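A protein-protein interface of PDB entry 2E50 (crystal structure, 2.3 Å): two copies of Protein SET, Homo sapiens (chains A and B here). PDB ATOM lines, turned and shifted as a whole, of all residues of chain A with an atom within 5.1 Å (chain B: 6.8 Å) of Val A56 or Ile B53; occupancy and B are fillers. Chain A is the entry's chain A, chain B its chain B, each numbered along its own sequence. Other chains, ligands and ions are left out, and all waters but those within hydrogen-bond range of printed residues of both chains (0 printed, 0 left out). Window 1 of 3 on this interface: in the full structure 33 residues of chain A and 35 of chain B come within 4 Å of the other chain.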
ATOM      1  N   GLU A  52     -25.036  11.147   3.528  1.00  0.00           N
ATOM      2  CA  GLU A  52     -25.206   9.735   3.221  1.00  0.00           C
ATOM      3  C   GLU A  52     -25.650   8.971   4.444  1.00  0.00           C
ATOM      4  O   GLU A  52     -26.540   8.137   4.348  1.00  0.00           O
ATOM      5  CB  GLU A  52     -23.970   9.118   2.551  1.00  0.00           C
ATOM      6  CG  GLU A  52     -23.920   9.423   1.045  1.00  0.00           C
ATOM      7  CD  GLU A  52     -22.785   8.727   0.303  1.00  0.00           C
ATOM      8  OE1 GLU A  52     -22.540   7.532   0.517  1.00  0.00           O
ATOM      9  OE2 GLU A  52     -22.158   9.364  -0.553  1.00  0.00           O
ATOM     10  N   ILE A  53     -25.078   9.295   5.601  1.00  0.00           N
ATOM     11  CA  ILE A  53     -25.376   8.576   6.823  1.00  0.00           C
ATOM     12  C   ILE A  53     -26.825   8.892   7.235  1.00  0.00           C
ATOM     13  O   ILE A  53     -27.573   8.011   7.610  1.00  0.00           O
ATOM     14  CB  ILE A  53     -24.389   8.962   7.923  1.00  0.00           C
ATOM     15  CG1 ILE A  53     -23.038   8.254   7.655  1.00  0.00           C
ATOM     16  CG2 ILE A  53     -24.977   8.542   9.327  1.00  0.00           C
ATOM     17  CD1 ILE A  53     -21.828   8.868   8.230  1.00  0.00           C
ATOM     18  N   LEU A  54     -27.198  10.175   7.145  1.00  0.00           N
ATOM     19  CA  LEU A  54     -28.561  10.607   7.385  1.00  0.00           C
ATOM     20  C   LEU A  54     -29.575   9.902   6.469  1.00  0.00           C
ATOM     21  O   LEU A  54     -30.616   9.556   6.954  1.00  0.00           O
ATOM     22  CB  LEU A  54     -28.689  12.148   7.362  1.00  0.00           C
ATOM     23  CG  LEU A  54     -27.928  12.824   8.547  1.00  0.00           C
ATOM     24  CD1 LEU A  54     -27.898  14.356   8.468  1.00  0.00           C
ATOM     25  CD2 LEU A  54     -28.397  12.388   9.963  1.00  0.00           C
ATOM     26  N   LYS A  55     -29.263   9.653   5.184  1.00  0.00           N
ATOM     27  CA  LYS A  55     -30.179   8.909   4.294  1.00  0.00           C
ATOM     28  C   LYS A  55     -30.314   7.433   4.739  1.00  0.00           C
ATOM     29  O   LYS A  55     -31.411   6.876   4.731  1.00  0.00           O
ATOM     30  CB  LYS A  55     -29.739   8.950   2.825  1.00  0.00           C
ATOM     31  CG  LYS A  55     -29.674  10.371   2.172  1.00  0.00           C
ATOM     32  CD  LYS A  55     -29.211  10.315   0.679  1.00  0.00           C
ATOM     33  CE  LYS A  55     -28.638  11.670   0.123  1.00  0.00           C
ATOM     34  NZ  LYS A  55     -27.154  11.629  -0.289  1.00  0.00           N
ATOM     35  N   VAL A  56     -29.197   6.805   5.093  1.00  0.00           N
ATOM     36  CA  VAL A  56     -29.215   5.456   5.636  1.00  0.00           C
ATOM     37  C   VAL A  56     -30.112   5.430   6.935  1.00  0.00           C
ATOM     38  O   VAL A  56     -30.959   4.565   7.113  1.00  0.00           O
ATOM     39  CB  VAL A  56     -27.763   4.944   5.938  1.00  0.00           C
ATOM     40  CG1 VAL A  56     -27.777   3.588   6.701  1.00  0.00           C
ATOM     41  CG2 VAL A  56     -26.906   4.846   4.661  1.00  0.00           C
ATOM     42  N   GLU A  57     -29.904   6.395   7.815  1.00  0.00           N
ATOM     43  CA  GLU A  57     -30.595   6.421   9.104  1.00  0.00           C
ATOM     44  C   GLU A  57     -32.110   6.623   8.913  1.00  0.00           C
ATOM     45  O   GLU A  57     -32.896   5.972   9.587  1.00  0.00           O
ATOM     46  CB  GLU A  57     -30.008   7.535   9.984  1.00  0.00           C
ATOM     47  CG  GLU A  57     -30.742   7.807  11.321  1.00  0.00           C
ATOM     48  CD  GLU A  57     -30.477   6.728  12.368  1.00  0.00           C
ATOM     49  OE1 GLU A  57     -29.811   5.723  12.050  1.00  0.00           O
ATOM     50  OE2 GLU A  57     -30.965   6.865  13.509  1.00  0.00           O
ATOM     51  N   GLN A  58     -32.498   7.499   7.999  1.00  0.00           N
ATOM     52  CA  GLN A  58     -33.872   7.741   7.695  1.00  0.00           C
ATOM     53  C   GLN A  58     -34.489   6.470   7.142  1.00  0.00           C
ATOM     54  O   GLN A  58     -35.567   6.087   7.552  1.00  0.00           O
ATOM     55  CB  GLN A  58     -34.035   8.933   6.726  1.00  0.00           C
ATOM     56  CG  GLN A  58     -35.509   9.348   6.525  1.00  0.00           C
ATOM     57  CD  GLN A  58     -35.794  10.220   5.291  1.00  0.00           C
ATOM     58  OE1 GLN A  58     -34.935  10.389   4.392  1.00  0.00           O
ATOM     59  NE2 GLN A  58     -37.015  10.753   5.222  1.00  0.00           N
ATOM     60  N   LYS A  59     -33.797   5.774   6.249  1.00  0.00           N
ATOM     61  CA  LYS A  59     -34.372   4.571   5.664  1.00  0.00           C
ATOM     62  C   LYS A  59     -34.672   3.433   6.694  1.00  0.00           C
ATOM     63  O   LYS A  59     -35.728   2.843   6.703  1.00  0.00           O
ATOM     64  CB  LYS A  59     -33.450   4.080   4.544  1.00  0.00           C
ATOM     65  CG  LYS A  59     -33.784   2.713   4.033  1.00  0.00           C
ATOM     66  CD  LYS A  59     -32.663   2.187   3.114  1.00  0.00           C
ATOM     67  CE  LYS A  59     -33.043   0.796   2.570  1.00  0.00           C
ATOM     68  NZ  LYS A  59     -32.000   0.172   1.702  1.00  0.00           N
ATOM     69  N   TYR A  60     -33.705   3.124   7.529  1.00  0.00           N
ATOM     70  CA  TYR A  60     -33.838   2.073   8.519  1.00  0.00           C
ATOM     71  C   TYR A  60     -34.692   2.485   9.705  1.00  0.00           C
ATOM     72  O   TYR A  60     -35.227   1.640  10.422  1.00  0.00           O
ATOM     73  CB  TYR A  60     -32.453   1.581   8.970  1.00  0.00           C
ATOM     74  CG  TYR A  60     -31.829   0.723   7.872  1.00  0.00           C
ATOM     75  CD1 TYR A  60     -30.910   1.264   6.951  1.00  0.00           C
ATOM     76  CD2 TYR A  60     -32.180  -0.602   7.736  1.00  0.00           C
ATOM     77  CE1 TYR A  60     -30.376   0.475   5.947  1.00  0.00           C
ATOM     78  CE2 TYR A  60     -31.651  -1.404   6.732  1.00  0.00           C
ATOM     79  CZ  TYR A  60     -30.753  -0.874   5.855  1.00  0.00           C
ATOM     80  OH  TYR A  60     -30.247  -1.701   4.854  1.00  0.00           O
ATOM     81  N   ASN A  61     -34.848   3.784   9.892  1.00  0.00           N
ATOM     82  CA  ASN A  61     -35.692   4.251  10.954  1.00  0.00           C
ATOM     83  C   ASN A  61     -37.118   3.921  10.595  1.00  0.00           C
ATOM     84  O   ASN A  61     -37.861   3.481  11.458  1.00  0.00           O
ATOM     85  CB  ASN A  61     -35.479   5.745  11.190  1.00  0.00           C
ATOM     86  CG  ASN A  61     -34.423   5.994  12.241  1.00  0.00           C
ATOM     87  OD1 ASN A  61     -34.097   7.142  12.586  1.00  0.00           O
ATOM     88  ND2 ASN A  61     -33.880   4.896  12.776  1.00  0.00           N
ATOM     89  N   GLN B  48     -28.121  -4.256   9.810  1.00  0.00           N
ATOM     90  CA  GLN B  48     -28.021  -3.705   8.460  1.00  0.00           C
ATOM     91  C   GLN B  48     -27.686  -2.194   8.496  1.00  0.00           C
ATOM     92  O   GLN B  48     -26.835  -1.753   7.766  1.00  0.00           O
ATOM     93  CB  GLN B  48     -29.268  -3.954   7.643  1.00  0.00           C
ATOM     94  CG  GLN B  48     -29.440  -5.381   7.252  1.00  0.00           C
ATOM     95  CD  GLN B  48     -30.865  -5.795   6.841  1.00  0.00           C
ATOM     96  OE1 GLN B  48     -31.085  -6.948   6.492  1.00  0.00           O
ATOM     97  NE2 GLN B  48     -31.805  -4.884   6.868  1.00  0.00           N
ATOM     98  N   ALA B  49     -28.327  -1.430   9.362  1.00  0.00           N
ATOM     99  CA  ALA B  49     -28.072   0.021   9.450  1.00  0.00           C
ATOM    100  C   ALA B  49     -26.641   0.350   9.821  1.00  0.00           C
ATOM    101  O   ALA B  49     -26.031   1.179   9.178  1.00  0.00           O
ATOM    102  CB  ALA B  49     -29.028   0.698  10.412  1.00  0.00           C
ATOM    103  N   SER B  50     -26.137  -0.304  10.857  1.00  0.00           N
ATOM    104  CA  SER B  50     -24.754  -0.234  11.252  1.00  0.00           C
ATOM    105  C   SER B  50     -23.736  -0.555  10.169  1.00  0.00           C
ATOM    106  O   SER B  50     -22.711   0.089  10.126  1.00  0.00           O
ATOM    107  CB  SER B  50     -24.475  -1.188  12.407  1.00  0.00           C
ATOM    108  OG  SER B  50     -24.744  -0.424  13.560  1.00  0.00           O
ATOM    109  N   GLU B  51     -24.016  -1.601   9.393  1.00  0.00           N
ATOM    110  CA  GLU B  51     -23.183  -2.006   8.298  1.00  0.00           C
ATOM    111  C   GLU B  51     -23.183  -0.934   7.202  1.00  0.00           C
ATOM    112  O   GLU B  51     -22.141  -0.626   6.715  1.00  0.00           O
ATOM    113  CB  GLU B  51     -23.572  -3.387   7.737  1.00  0.00           C
ATOM    114  CG  GLU B  51     -23.402  -4.536   8.802  1.00  0.00           C
ATOM    115  CD  GLU B  51     -24.073  -5.896   8.422  1.00  0.00           C
ATOM    116  OE1 GLU B  51     -24.783  -5.994   7.378  1.00  0.00           O
ATOM    117  OE2 GLU B  51     -23.892  -6.870   9.195  1.00  0.00           O
ATOM    118  N   GLU B  52     -24.339  -0.366   6.853  1.00  0.00           N
ATOM    119  CA  GLU B  52     -24.406   0.636   5.758  1.00  0.00           C
ATOM    120  C   GLU B  52     -23.751   1.932   6.189  1.00  0.00           C
ATOM    121  O   GLU B  52     -23.167   2.631   5.382  1.00  0.00           O
ATOM    122  CB  GLU B  52     -25.846   0.869   5.270  1.00  0.00           C
ATOM    123  CG  GLU B  52     -26.352  -0.195   4.257  1.00  0.00           C
ATOM    124  CD  GLU B  52     -27.738   0.155   3.674  1.00  0.00           C
ATOM    125  OE1 GLU B  52     -27.954   1.342   3.249  1.00  0.00           O
ATOM    126  OE2 GLU B  52     -28.619  -0.773   3.604  1.00  0.00           O
ATOM    127  N   ILE B  53     -23.852   2.254   7.468  1.00  0.00           N
ATOM    128  CA  ILE B  53     -23.209   3.436   7.980  1.00  0.00           C
ATOM    129  C   ILE B  53     -21.677   3.264   7.976  1.00  0.00           C
ATOM    130  O   ILE B  53     -20.966   4.132   7.540  1.00  0.00           O
ATOM    131  CB  ILE B  53     -23.751   3.821   9.364  1.00  0.00           C
ATOM    132  CG1 ILE B  53     -25.126   4.445   9.166  1.00  0.00           C
ATOM    133  CG2 ILE B  53     -22.841   4.849  10.016  1.00  0.00           C
ATOM    134  CD1 ILE B  53     -25.901   4.664  10.393  1.00  0.00           C
ATOM    135  N   LEU B  54     -21.210   2.112   8.435  1.00  0.00           N
ATOM    136  CA  LEU B  54     -19.829   1.800   8.458  1.00  0.00           C
ATOM    137  C   LEU B  54     -19.219   1.843   7.042  1.00  0.00           C
ATOM    138  O   LEU B  54     -18.185   2.416   6.856  1.00  0.00           O
ATOM    139  CB  LEU B  54     -19.649   0.448   9.139  1.00  0.00           C
ATOM    140  CG  LEU B  54     -18.229  -0.061   9.296  1.00  0.00           C
ATOM    141  CD1 LEU B  54     -17.568   0.606  10.466  1.00  0.00           C
ATOM    142  CD2 LEU B  54     -18.319  -1.604   9.465  1.00  0.00           C
ATOM    143  N   LYS B  55     -19.913   1.319   6.045  1.00  0.00           N
ATOM    144  CA  LYS B  55     -19.464   1.416   4.694  1.00  0.00           C
ATOM    145  C   LYS B  55     -19.367   2.855   4.206  1.00  0.00           C
ATOM    146  O   LYS B  55     -18.516   3.138   3.367  1.00  0.00           O
ATOM    147  CB  LYS B  55     -20.355   0.630   3.719  1.00  0.00           C
ATOM    148  CG  LYS B  55     -20.595  -0.826   4.054  1.00  0.00           C
ATOM    149  CD  LYS B  55     -19.406  -1.726   3.706  1.00  0.00           C
ATOM    150  CE  LYS B  55     -19.886  -3.188   3.537  1.00  0.00           C
ATOM    151  NZ  LYS B  55     -20.796  -3.700   4.653  1.00  0.00           N
ATOM    152  N   VAL B  56     -20.250   3.741   4.666  1.00  0.00           N
ATOM    153  CA  VAL B  56     -20.158   5.150   4.298  1.00  0.00           C
ATOM    154  C   VAL B  56     -18.889   5.741   4.857  1.00  0.00           C
ATOM    155  O   VAL B  56     -18.183   6.487   4.183  1.00  0.00           O
ATOM    156  CB  VAL B  56     -21.351   6.028   4.780  1.00  0.00           C
ATOM    157  CG1 VAL B  56     -21.049   7.604   4.500  1.00  0.00           C
ATOM    158  CG2 VAL B  56     -22.670   5.588   4.161  1.00  0.00           C
ATOM    159  N   GLU B  57     -18.621   5.443   6.112  1.00  0.00           N
ATOM    160  CA  GLU B  57     -17.421   5.934   6.772  1.00  0.00           C
ATOM    161  C   GLU B  57     -16.133   5.387   6.155  1.00  0.00           C
ATOM    162  O   GLU B  57     -15.154   6.113   6.049  1.00  0.00           O
ATOM    163  CB  GLU B  57     -17.483   5.581   8.259  1.00  0.00           C
ATOM    164  CG  GLU B  57     -18.381   6.562   9.041  1.00  0.00           C
ATOM    165  CD  GLU B  57     -18.718   6.064  10.459  1.00  0.00           C
ATOM    166  OE1 GLU B  57     -19.296   6.823  11.286  1.00  0.00           O
ATOM    167  OE2 GLU B  57     -18.406   4.899  10.743  1.00  0.00           O
ATOM    168  N   GLN B  58     -16.136   4.099   5.794  1.00  0.00           N
ATOM    169  CA  GLN B  58     -15.014   3.500   5.098  1.00  0.00           C
ATOM    170  C   GLN B  58     -14.736   4.170   3.740  1.00  0.00           C
ATOM    171  O   GLN B  58     -13.608   4.483   3.423  1.00  0.00           O
ATOM    172  CB  GLN B  58     -15.267   2.005   4.880  1.00  0.00           C
ATOM    173  CG  GLN B  58     -15.242   1.217   6.152  1.00  0.00           C
ATOM    174  CD  GLN B  58     -15.785  -0.190   5.996  1.00  0.00           C
ATOM    175  OE1 GLN B  58     -16.339  -0.570   4.954  1.00  0.00           O
ATOM    176  NE2 GLN B  58     -15.602  -0.987   7.029  1.00  0.00           N
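OE2 of Glu B52 sits close to OH of Tyr A60, at 2.3 Å.
NZ of Lys A59 is in salt-bridge range of OE2 of Glu B52, 3.99 Å away.
Among the printed residues, pairs that only touch across the chains: Tyr A60 with Gln B48 (3.5 Å), Val A56 with Glu B52 (3.6 Å), Val A56 with Ile B53 (3.7 Å), Tyr A60 with Ala B49 (3.8 Å), Ile A53 with Val B56 (3.8 Å), Glu A52 with Val B56 (3.8 Å) and Val A56 with Ala B49 (3.9 Å).
Val A56 touches just these residues of chain B: Ala B49 (3.9 Å), Glu B52 (3.6 Å) and Ile B53 (3.7 Å).
Ile B53 touches just one residue of chain A: Val A56 (3.7 Å).
Printed residues of chain A within 4 Å of Ala B49: Val A56 (3.9 Å) and Tyr A60 (3.8 Å).
Printed residues of chain A within 4 Å of Glu B52: Val A56, Lys A59 and Tyr A60.
Of the printed residues of chain B, Ile A53 touches Val B56 (3.8 Å).
Of the printed residues of chain B, Glu A52 touches Val B56 (3.8 Å).
The nearest printed residue of chain A that does not touch Glu B52 is Ile A53 (6.1 Å).
Among the printed residues, Asp or Glu carboxylates within 4 Å of a Lys or Arg side-chain nitrogen of the other chain: Lys A59 with Glu B52.
Glu A52 touches Val B56, and with the chains exchanged Val A56 touches Glu B52.
Ile A53 touches Val B56, and with the chains exchanged Val A56 touches Ile B53.
7 positions are printed for both chains.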
